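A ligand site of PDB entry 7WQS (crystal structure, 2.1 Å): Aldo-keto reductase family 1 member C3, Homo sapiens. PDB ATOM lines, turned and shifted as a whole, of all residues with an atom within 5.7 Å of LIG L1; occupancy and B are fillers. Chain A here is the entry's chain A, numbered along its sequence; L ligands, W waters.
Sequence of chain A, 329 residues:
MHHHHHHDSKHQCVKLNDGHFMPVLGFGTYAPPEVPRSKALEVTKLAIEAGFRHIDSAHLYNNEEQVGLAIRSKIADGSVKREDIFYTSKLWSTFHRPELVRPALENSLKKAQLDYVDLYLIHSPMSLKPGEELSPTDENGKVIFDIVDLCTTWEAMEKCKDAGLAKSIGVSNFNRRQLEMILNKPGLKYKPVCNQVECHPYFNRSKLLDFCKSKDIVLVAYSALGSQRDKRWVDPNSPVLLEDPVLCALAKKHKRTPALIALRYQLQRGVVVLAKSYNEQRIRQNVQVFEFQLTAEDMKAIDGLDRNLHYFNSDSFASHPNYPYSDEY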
ATOM      1  N   LEU A  60       4.467  -3.852  11.571  1.00  0.00           N
ATOM      2  CA  LEU A  60       3.497  -3.817  12.654  1.00  0.00           C
ATOM      3  C   LEU A  60       2.634  -5.070  12.697  1.00  0.00           C
ATOM      4  O   LEU A  60       2.208  -5.491  13.779  1.00  0.00           O
ATOM      5  CB  LEU A  60       2.604  -2.577  12.515  1.00  0.00           C
ATOM      6  CG  LEU A  60       1.481  -2.381  13.536  1.00  0.00           C
ATOM      7  CD1 LEU A  60       2.048  -1.930  14.871  1.00  0.00           C
ATOM      8  CD2 LEU A  60       0.459  -1.385  13.027  1.00  0.00           C
ATOM      9  N   TRP A  92       7.675   1.169  10.599  1.00  0.00           N
ATOM     10  CA  TRP A  92       6.838   1.542  11.734  1.00  0.00           C
ATOM     11  C   TRP A  92       7.359   2.814  12.393  1.00  0.00           C
ATOM     12  O   TRP A  92       8.529   3.192  12.258  1.00  0.00           O
ATOM     13  CB  TRP A  92       6.743   0.408  12.755  1.00  0.00           C
ATOM     14  CG  TRP A  92       5.765   0.732  13.866  1.00  0.00           C
ATOM     15  CD1 TRP A  92       6.007   0.661  15.204  1.00  0.00           C
ATOM     16  CD2 TRP A  92       4.418   1.208  13.722  1.00  0.00           C
ATOM     17  NE1 TRP A  92       4.888   1.058  15.900  1.00  0.00           N
ATOM     18  CE2 TRP A  92       3.904   1.386  15.011  1.00  0.00           C
ATOM     19  CE3 TRP A  92       3.598   1.478  12.618  1.00  0.00           C
ATOM     20  CZ2 TRP A  92       2.604   1.838  15.234  1.00  0.00           C
ATOM     21  CZ3 TRP A  92       2.310   1.924  12.837  1.00  0.00           C
ATOM     22  CH2 TRP A  92       1.819   2.102  14.142  1.00  0.00           C
ATOM     23  N   SER A  93       6.464   3.479  13.121  1.00  0.00           N
ATOM     24  CA  SER A  93       6.687   4.825  13.649  1.00  0.00           C
ATOM     25  C   SER A  93       7.782   4.885  14.707  1.00  0.00           C
ATOM     26  O   SER A  93       8.214   5.987  15.049  1.00  0.00           O
ATOM     27  CB  SER A  93       5.386   5.373  14.224  1.00  0.00           C
ATOM     28  OG  SER A  93       4.354   5.313  13.262  1.00  0.00           O
ATOM     29  N   HIS A 123       4.667   4.156   7.513  1.00  0.00           N
ATOM     30  CA  HIS A 123       3.355   3.659   7.924  1.00  0.00           C
ATOM     31  C   HIS A 123       2.459   4.777   8.424  1.00  0.00           C
ATOM     32  O   HIS A 123       1.237   4.764   8.205  1.00  0.00           O
ATOM     33  CB  HIS A 123       3.515   2.587   8.992  1.00  0.00           C
ATOM     34  CG  HIS A 123       2.353   1.636   9.090  1.00  0.00           C
ATOM     35  ND1 HIS A 123       2.510   0.296   9.363  1.00  0.00           N
ATOM     36  CD2 HIS A 123       1.029   1.842   8.956  1.00  0.00           C
ATOM     37  CE1 HIS A 123       1.331  -0.283   9.384  1.00  0.00           C
ATOM     38  NE2 HIS A 123       0.404   0.625   9.141  1.00  0.00           N
ATOM     39  N   SER A 124       3.043   5.766   9.109  1.00  0.00           N
ATOM     40  CA  SER A 124       2.258   6.828   9.731  1.00  0.00           C
ATOM     41  C   SER A 124       3.167   8.038   9.902  1.00  0.00           C
ATOM     42  O   SER A 124       4.378   7.880  10.048  1.00  0.00           O
ATOM     43  CB  SER A 124       1.702   6.381  11.088  1.00  0.00           C
ATOM     44  OG  SER A 124       1.134   7.462  11.796  1.00  0.00           O
ATOM     45  N   PRO A 125       2.609   9.259   9.878  1.00  0.00           N
ATOM     46  CA  PRO A 125       3.425  10.440  10.189  1.00  0.00           C
ATOM     47  C   PRO A 125       3.646  10.650  11.682  1.00  0.00           C
ATOM     48  O   PRO A 125       4.482  11.492  12.040  1.00  0.00           O
ATOM     49  CB  PRO A 125       2.604  11.580   9.587  1.00  0.00           C
ATOM     50  CG  PRO A 125       1.198  11.109   9.659  1.00  0.00           C
ATOM     51  CD  PRO A 125       1.252   9.612   9.432  1.00  0.00           C
ATOM     52  N   MET A 126       2.944   9.909  12.536  1.00  0.00           N
ATOM     53  CA  MET A 126       3.015  10.121  13.982  1.00  0.00           C
ATOM     54  C   MET A 126       4.168   9.307  14.542  1.00  0.00           C
ATOM     55  O   MET A 126       4.037   8.115  14.854  1.00  0.00           O
ATOM     56  CB  MET A 126       1.692   9.732  14.639  1.00  0.00           C
ATOM     57  CG  MET A 126       0.505  10.579  14.210  1.00  0.00           C
ATOM     58  SD  MET A 126      -0.995  10.178  15.111  1.00  0.00           S
ATOM     59  CE  MET A 126      -1.353   8.536  14.473  1.00  0.00           C
ATOM     60  N   LEU A 128       6.920   7.760  17.037  1.00  0.00           N
ATOM     61  CA  LEU A 128       6.839   7.218  18.388  1.00  0.00           C
ATOM     62  C   LEU A 128       8.246   6.973  18.913  1.00  0.00           C
ATOM     63  O   LEU A 128       9.220   6.973  18.162  1.00  0.00           O
ATOM     64  CB  LEU A 128       6.020   5.912  18.417  1.00  0.00           C
ATOM     65  CG  LEU A 128       4.619   5.995  17.808  1.00  0.00           C
ATOM     66  CD1 LEU A 128       3.936   4.636  17.828  1.00  0.00           C
ATOM     67  CD2 LEU A 128       3.776   7.033  18.546  1.00  0.00           C
ATOM     68  N   LEU A 134       6.665  -1.844  19.911  1.00  0.00           N
ATOM     69  CA  LEU A 134       5.810  -1.237  18.899  1.00  0.00           C
ATOM     70  C   LEU A 134       4.925  -0.144  19.503  1.00  0.00           C
ATOM     71  O   LEU A 134       4.707   0.904  18.876  1.00  0.00           O
ATOM     72  CB  LEU A 134       4.959  -2.301  18.219  1.00  0.00           C
ATOM     73  CG  LEU A 134       5.704  -3.305  17.316  1.00  0.00           C
ATOM     74  CD1 LEU A 134       4.805  -3.779  16.185  1.00  0.00           C
ATOM     75  CD2 LEU A 134       6.988  -2.701  16.765  1.00  0.00           C
ATOM     76  N   SER A 135       4.410  -0.371  20.713  1.00  0.00           N
ATOM     77  CA  SER A 135       3.555   0.584  21.416  1.00  0.00           C
ATOM     78  C   SER A 135       4.219   0.971  22.737  1.00  0.00           C
ATOM     79  O   SER A 135       3.797   0.503  23.801  1.00  0.00           O
ATOM     80  CB  SER A 135       2.164   0.009  21.658  1.00  0.00           C
ATOM     81  OG  SER A 135       1.531  -0.345  20.440  1.00  0.00           O
ATOM     82  N   VAL A 143       0.742   6.279  25.111  1.00  0.00           N
ATOM     83  CA  VAL A 143       1.735   6.056  24.064  1.00  0.00           C
ATOM     84  C   VAL A 143       2.713   7.230  24.030  1.00  0.00           C
ATOM     85  O   VAL A 143       2.303   8.399  24.044  1.00  0.00           O
ATOM     86  CB  VAL A 143       1.036   5.862  22.712  1.00  0.00           C
ATOM     87  CG1 VAL A 143       2.045   5.865  21.576  1.00  0.00           C
ATOM     88  CG2 VAL A 143       0.228   4.568  22.713  1.00  0.00           C
ATOM     89  N   ASN A 173      -1.071   7.367   5.518  1.00  0.00           N
ATOM     90  CA  ASN A 173      -1.765   8.179   6.515  1.00  0.00           C
ATOM     91  C   ASN A 173      -1.274   9.620   6.544  1.00  0.00           C
ATOM     92  O   ASN A 173      -1.381  10.296   7.572  1.00  0.00           O
ATOM     93  CB  ASN A 173      -1.652   7.565   7.922  1.00  0.00           C
ATOM     94  CG  ASN A 173      -2.342   6.218   8.013  1.00  0.00           C
ATOM     95  OD1 ASN A 173      -3.560   6.118   7.870  1.00  0.00           O
ATOM     96  ND2 ASN A 173      -1.562   5.172   8.264  1.00  0.00           N
ATOM     97  N   GLU A 198      -7.102   5.529   4.756  1.00  0.00           N
ATOM     98  CA  GLU A 198      -8.452   4.982   4.894  1.00  0.00           C
ATOM     99  C   GLU A 198      -9.367   5.629   3.869  1.00  0.00           C
ATOM    100  O   GLU A 198      -9.456   6.851   3.789  1.00  0.00           O
ATOM    101  CB  GLU A 198      -9.001   5.215   6.304  1.00  0.00           C
ATOM    102  CG  GLU A 198     -10.312   4.481   6.540  1.00  0.00           C
ATOM    103  CD  GLU A 198     -10.875   4.679   7.933  1.00  0.00           C
ATOM    104  OE1 GLU A 198     -10.100   4.967   8.869  1.00  0.00           O
ATOM    105  OE2 GLU A 198     -12.107   4.538   8.086  1.00  0.00           O
ATOM    106  N   TYR A 222      -7.278   1.754   2.136  1.00  0.00           N
ATOM    107  CA  TYR A 222      -7.469   0.684   3.110  1.00  0.00           C
ATOM    108  C   TYR A 222      -8.790   0.878   3.838  1.00  0.00           C
ATOM    109  O   TYR A 222      -9.418   1.943   3.763  1.00  0.00           O
ATOM    110  CB  TYR A 222      -6.283   0.594   4.098  1.00  0.00           C
ATOM    111  CG  TYR A 222      -6.139   1.683   5.152  1.00  0.00           C
ATOM    112  CD1 TYR A 222      -7.020   1.775   6.221  1.00  0.00           C
ATOM    113  CD2 TYR A 222      -5.086   2.592   5.105  1.00  0.00           C
ATOM    114  CE1 TYR A 222      -6.873   2.745   7.196  1.00  0.00           C
ATOM    115  CE2 TYR A 222      -4.933   3.563   6.071  1.00  0.00           C
ATOM    116  CZ  TYR A 222      -5.835   3.636   7.110  1.00  0.00           C
ATOM    117  OH  TYR A 222      -5.689   4.605   8.084  1.00  0.00           O
ATOM    118  N   SER A 223      -9.220  -0.183   4.527  1.00  0.00           N
ATOM    119  CA  SER A 223     -10.562  -0.251   5.097  1.00  0.00           C
ATOM    120  C   SER A 223     -11.626   0.026   4.042  1.00  0.00           C
ATOM    121  O   SER A 223     -12.681   0.609   4.327  1.00  0.00           O
ATOM    122  CB  SER A 223     -10.718   0.688   6.295  1.00  0.00           C
ATOM    123  OG  SER A 223      -9.912   0.270   7.378  1.00  0.00           O
ATOM    124  N   TRP A 233     -10.489  -0.168  18.593  1.00  0.00           N
ATOM    125  CA  TRP A 233     -10.467   1.193  17.979  1.00  0.00           C
ATOM    126  C   TRP A 233     -11.803   1.618  17.348  1.00  0.00           C
ATOM    127  O   TRP A 233     -11.946   2.767  17.004  1.00  0.00           O
ATOM    128  CB  TRP A 233      -9.411   1.266  16.876  1.00  0.00           C
ATOM    129  CG  TRP A 233      -8.116   0.573  17.135  1.00  0.00           C
ATOM    130  CD1 TRP A 233      -7.137   0.956  17.985  1.00  0.00           C
ATOM    131  CD2 TRP A 233      -7.636  -0.607  16.497  1.00  0.00           C
ATOM    132  NE1 TRP A 233      -6.107   0.064  17.957  1.00  0.00           N
ATOM    133  CE2 TRP A 233      -6.388  -0.901  17.059  1.00  0.00           C
ATOM    134  CE3 TRP A 233      -8.149  -1.450  15.513  1.00  0.00           C
ATOM    135  CZ2 TRP A 233      -5.640  -1.999  16.667  1.00  0.00           C
ATOM    136  CZ3 TRP A 233      -7.402  -2.527  15.135  1.00  0.00           C
ATOM    137  CH2 TRP A 233      -6.184  -2.826  15.714  1.00  0.00           C
ATOM    138  N   PHE A 312     -11.006   4.111  12.202  1.00  0.00           N
ATOM    139  CA  PHE A 312      -9.964   4.295  13.203  1.00  0.00           C
ATOM    140  C   PHE A 312     -10.116   5.676  13.839  1.00  0.00           C
ATOM    141  O   PHE A 312     -10.007   6.695  13.146  1.00  0.00           O
ATOM    142  CB  PHE A 312      -8.568   4.156  12.602  1.00  0.00           C
ATOM    143  CG  PHE A 312      -7.484   4.691  13.491  1.00  0.00           C
ATOM    144  CD1 PHE A 312      -7.032   3.950  14.574  1.00  0.00           C
ATOM    145  CD2 PHE A 312      -6.929   5.943  13.273  1.00  0.00           C
ATOM    146  CE1 PHE A 312      -6.036   4.436  15.404  1.00  0.00           C
ATOM    147  CE2 PHE A 312      -5.933   6.429  14.102  1.00  0.00           C
ATOM    148  CZ  PHE A 312      -5.487   5.675  15.168  1.00  0.00           C
ATOM    149  N   PHE A 317      -4.285   9.766  20.134  1.00  0.00           N
ATOM    150  CA  PHE A 317      -3.392  10.211  19.047  1.00  0.00           C
ATOM    151  C   PHE A 317      -3.791  11.602  18.556  1.00  0.00           C
ATOM    152  O   PHE A 317      -2.973  12.209  17.889  1.00  0.00           O
ATOM    153  CB  PHE A 317      -3.224   9.162  17.952  1.00  0.00           C
ATOM    154  CG  PHE A 317      -2.582   7.866  18.375  1.00  0.00           C
ATOM    155  CD1 PHE A 317      -1.208   7.728  18.443  1.00  0.00           C
ATOM    156  CD2 PHE A 317      -3.349   6.756  18.660  1.00  0.00           C
ATOM    157  CE1 PHE A 317      -0.618   6.534  18.819  1.00  0.00           C
ATOM    158  CE2 PHE A 317      -2.764   5.567  19.057  1.00  0.00           C
ATOM    159  CZ  PHE A 317      -1.399   5.455  19.137  1.00  0.00           C
ATOM    160  N   PRO A 324      -3.006  13.094  11.530  1.00  0.00           N
ATOM    161  CA  PRO A 324      -3.307  13.462  10.184  1.00  0.00           C
ATOM    162  C   PRO A 324      -4.706  14.031  10.004  1.00  0.00           C
ATOM    163  O   PRO A 324      -4.913  14.704   9.100  1.00  0.00           O
ATOM    164  CB  PRO A 324      -3.101  12.161   9.439  1.00  0.00           C
ATOM    165  CG  PRO A 324      -3.456  11.116  10.410  1.00  0.00           C
ATOM    166  CD  PRO A 324      -3.099  11.686  11.760  1.00  0.00           C
ATOM    167  N   TYR A 325      -5.610  13.713  10.904  1.00  0.00           N
ATOM    168  CA  TYR A 325      -6.978  14.225  10.813  1.00  0.00           C
ATOM    169  C   TYR A 325      -7.088  15.561  11.546  1.00  0.00           C
ATOM    170  O   TYR A 325      -7.880  15.747  12.472  1.00  0.00           O
ATOM    171  CB  TYR A 325      -7.974  13.201  11.344  1.00  0.00           C
ATOM    172  CG  TYR A 325      -7.912  11.874  10.627  1.00  0.00           C
ATOM    173  CD1 TYR A 325      -7.710  11.806   9.253  1.00  0.00           C
ATOM    174  CD2 TYR A 325      -8.061  10.680  11.324  1.00  0.00           C
ATOM    175  CE1 TYR A 325      -7.655  10.586   8.598  1.00  0.00           C
ATOM    176  CE2 TYR A 325      -8.012   9.458  10.677  1.00  0.00           C
ATOM    177  CZ  TYR A 325      -7.801   9.419   9.315  1.00  0.00           C
ATOM    178  OH  TYR A 325      -7.752   8.197   8.667  1.00  0.00           O
HETATM  179  N1  LIG L   1      -3.325   3.093  14.482  1.00  0.00           N
HETATM  180  C1  LIG L   1      -6.902   0.934  11.539  1.00  0.00           C
HETATM  181  C2  LIG L   1      -6.838   0.250  12.711  1.00  0.00           C
HETATM  182  C3  LIG L   1      -5.943   0.643  13.677  1.00  0.00           C
HETATM  183  C4  LIG L   1      -4.157   2.044  14.630  1.00  0.00           C
HETATM  184  C5  LIG L   1      -2.208   3.412  15.273  1.00  0.00           C
HETATM  185  C6  LIG L   1      -0.537   2.822  16.871  1.00  0.00           C
HETATM  186  C7  LIG L   1      -1.681   4.688  15.213  1.00  0.00           C
HETATM  187  C8  LIG L   1      -4.250   4.146  10.919  1.00  0.00           C
HETATM  188  C9  LIG L   1      -2.129   5.192  11.486  1.00  0.00           C
HETATM  189  C10 LIG L   1      -1.300   4.009  11.775  1.00  0.00           C
HETATM  190  C11 LIG L   1      -5.089   1.725  13.500  1.00  0.00           C
HETATM  191  C12 LIG L   1      -0.022   4.101  16.840  1.00  0.00           C
HETATM  192  C13 LIG L   1      -0.576   5.022  15.998  1.00  0.00           C
HETATM  193  C14 LIG L   1       1.319   1.817  18.024  1.00  0.00           C
HETATM  194  C15 LIG L   1      -3.411   5.341  11.124  1.00  0.00           C
HETATM  195  C16 LIG L   1      -3.635   6.708  11.005  1.00  0.00           C
HETATM  196  C17 LIG L   1      -4.872   7.427  10.606  1.00  0.00           C
HETATM  197  C18 LIG L   1      -5.189   2.432  12.293  1.00  0.00           C
HETATM  198  C19 LIG L   1      -6.112   2.030  11.330  1.00  0.00           C
HETATM  199  C20 LIG L   1      -1.659   2.482  16.135  1.00  0.00           C
HETATM  200  N2  LIG L   1      -2.553   7.364  11.263  1.00  0.00           N
HETATM  201  O1  LIG L   1      -4.322   3.471  12.181  1.00  0.00           O
HETATM  202  O2  LIG L   1      -4.143   1.368  15.642  1.00  0.00           O
HETATM  203  O3  LIG L   1      -0.055   1.848  17.702  1.00  0.00           O
HETATM  204  O4  LIG L   1      -1.572   6.410  11.576  1.00  0.00           O
HETATM  205  P1  LG2 L   2     -11.040  -4.484   4.917  1.00  0.00           P
HETATM  206  O1  LG2 L   2     -11.754  -3.138   5.087  1.00  0.00           O
HETATM  207  O2  LG2 L   2     -10.393  -4.549   3.532  1.00  0.00           O
HETATM  208  O3  LG2 L   2     -12.157  -5.702   5.080  1.00  0.00           O
HETATM  209  C1  LG2 L   2     -13.015  -5.619   6.240  1.00  0.00           C
HETATM  210  C2  LG2 L   2     -13.730  -6.979   6.436  1.00  0.00           C
HETATM  211  O4  LG2 L   2     -14.483  -7.223   5.373  1.00  0.00           O
HETATM  212  C3  LG2 L   2     -12.703  -8.104   6.454  1.00  0.00           C
HETATM  213  O5  LG2 L   2     -12.376  -8.403   7.718  1.00  0.00           O
HETATM  214  C4  LG2 L   2     -13.430  -9.315   5.767  1.00  0.00           C
HETATM  215  O6  LG2 L   2     -13.776 -10.333   6.811  1.00  0.00           O
HETATM  216  C5  LG2 L   2     -14.527  -8.841   5.218  1.00  0.00           C
HETATM  217  N1  LG2 L   2     -14.562  -9.171   3.817  1.00  0.00           N
HETATM  218  C6  LG2 L   2     -13.599  -9.331   2.896  1.00  0.00           C
HETATM  219  N2  LG2 L   2     -14.184  -9.637   1.721  1.00  0.00           N
HETATM  220  C7  LG2 L   2     -15.527  -9.670   1.922  1.00  0.00           C
HETATM  221  C8  LG2 L   2     -16.579  -9.921   1.065  1.00  0.00           C
HETATM  222  N3  LG2 L   2     -16.509 -10.255  -0.361  1.00  0.00           N
HETATM  223  N4  LG2 L   2     -17.838  -9.890   1.512  1.00  0.00           N
HETATM  224  C9  LG2 L   2     -18.082  -9.597   2.816  1.00  0.00           C
HETATM  225  N5  LG2 L   2     -17.049  -9.339   3.661  1.00  0.00           N
HETATM  226  C10 LG2 L   2     -15.765  -9.381   3.205  1.00  0.00           C
HETATM  227  O7  LG2 L   2      -9.895  -4.715   6.127  1.00  0.00           O
HETATM  228  P2  LG2 L   2      -8.835  -3.611   6.690  1.00  0.00           P
HETATM  229  O8  LG2 L   2      -7.904  -4.303   7.619  1.00  0.00           O
HETATM  230  O9  LG2 L   2      -9.526  -2.512   7.424  1.00  0.00           O
HETATM  231  O10 LG2 L   2      -8.002  -2.990   5.401  1.00  0.00           O
HETATM  232  C11 LG2 L   2      -7.450  -3.942   4.427  1.00  0.00           C
HETATM  233  C12 LG2 L   2      -5.905  -3.850   4.457  1.00  0.00           C
HETATM  234  O11 LG2 L   2      -5.546  -2.596   4.422  1.00  0.00           O
HETATM  235  C13 LG2 L   2      -5.346  -4.363   5.794  1.00  0.00           C
HETATM  236  O12 LG2 L   2      -5.208  -5.720   5.826  1.00  0.00           O
HETATM  237  C14 LG2 L   2      -3.975  -3.651   5.847  1.00  0.00           C
HETATM  238  O13 LG2 L   2      -3.019  -4.433   4.996  1.00  0.00           O
HETATM  239  C15 LG2 L   2      -4.192  -2.472   5.317  1.00  0.00           C
HETATM  240  N6  LG2 L   2      -4.323  -1.417   6.327  1.00  0.00           N
HETATM  241  C16 LG2 L   2      -3.392  -0.428   6.378  1.00  0.00           C
HETATM  242  C17 LG2 L   2      -3.491   0.577   7.342  1.00  0.00           C
HETATM  243  C18 LG2 L   2      -2.446   1.681   7.395  1.00  0.00           C
HETATM  244  O14 LG2 L   2      -2.381   2.390   8.355  1.00  0.00           O
HETATM  245  N7  LG2 L   2      -1.530   1.875   6.272  1.00  0.00           N
HETATM  246  C19 LG2 L   2      -4.519   0.580   8.227  1.00  0.00           C
HETATM  247  C20 LG2 L   2      -5.456  -0.402   8.172  1.00  0.00           C
HETATM  248  C21 LG2 L   2      -5.340  -1.406   7.209  1.00  0.00           C
HETATM  249  P3  LG2 L   2     -13.256 -11.891   6.578  1.00  0.00           P
HETATM  250  O15 LG2 L   2     -11.803 -11.973   6.888  1.00  0.00           O
HETATM  251  O16 LG2 L   2     -14.022 -12.821   7.480  1.00  0.00           O
HETATM  252  O17 LG2 L   2     -13.490 -12.272   5.136  1.00  0.00           O
HETATM  253  O   HOH W   1     -10.120   0.798  12.440  1.00  0.00           O
HETATM  254  O   HOH W   2      -9.550   1.920   9.779  1.00  0.00           O
HETATM  255  O   HOH W   3      -3.288  -1.061  14.028  1.00  0.00           O
HETATM  256  O   HOH W   4       2.291   6.128  14.759  1.00  0.00           O
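ND2 of Asn 173 lies within hydrogen-bond range of O14 of LG2 L2, 2.9 Å away.
The indole nitrogen (NE1) of Trp 233 lies within hydrogen-bond range of an oxygen (O2) of LIG L1 (3.3 Å).
NE2 of His 123 is in hydrogen-bond range of O14 of LG2 L2 (3.4 Å).
O10 of LG2 L2 sits at hydrogen-bond distance from N of Ser 223 (3.2 Å).
O4 of LIG L1 is in hydrogen-bond range of OG of Ser 124, 2.9 Å away.
An oxygen (O9) of LG2 L2 sits at hydrogen-bond distance from the side-chain hydroxyl of Ser 223.
The backbone carbonyl oxygen (O) of Met 126 sits close to the side-chain hydroxyl (OG) of Ser 93 (3.2 Å).
The indole nitrogen (NE1) of Trp 92 lies within hydrogen-bond range of the backbone carbonyl oxygen (O) of Leu 134, 3.0 Å away.
OD1 of Asn 173 is in hydrogen-bond range of OH of Tyr 222, at 2.6 Å.
The side-chain amide nitrogen of Asn 173 sits at hydrogen-bond distance from the backbone carbonyl oxygen of His 123 (2.8 Å).
The side-chain hydroxyl (OG) of Ser 124 lies within hydrogen-bond range of the backbone NH (N) of Met 126 (3.1 Å).
The backbone NH (N) of Leu 128 lies within hydrogen-bond range of the backbone carbonyl oxygen (O) of Ser 93 (3.0 Å).
Trp 92 touches LIG L1 (CZ2 to C14, 3.1 Å).
Met 126 touches LIG L1 (CE to O4, 3.6 Å).
Leu 128 touches LIG L1 (CD1 to C14, 3.9 Å).
Leu 134 touches LIG L1 (O to C14, 3.6 Å).
Ser 135 touches LIG L1 (OG to C14, 3.2 Å).
OD1 of Asn 173 touches C16 of LIG L1 (3.2 Å).
Tyr 222 touches LIG L1 (OH to C8, 3.2 Å).
Phe 312 touches LIG L1 (CE1 to C4, 3.1 Å).
Phe 317 touches LIG L1.
CG of Pro 324 touches N2 of LIG L1, 3.95 Å away.
Tyr 325 touches LIG L1.
Within 4 Å of LIG L1: Trp 92, Ser 124, Met 126, Leu 128, Leu 134, Ser 135, Asn 173, Tyr 222, Trp 233, Phe 312, Phe 317, Pro 324 and Tyr 325.
The nearest printed residue that does not touch LIG L1 is His 123 (4.3 Å).
Water W4 lies within hydrogen-bond range of the backbone carbonyl oxygen of Met 126 (2.6 Å), the side-chain hydroxyl of Ser 93 (2.7 Å) and the side-chain hydroxyl of Ser 124 (3.4 Å).
Water W2 lies within hydrogen-bond range of the side-chain hydroxyl of Ser 223 (2.9 Å) and the side-chain carboxylate of Glu 198 (3.2 Å).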
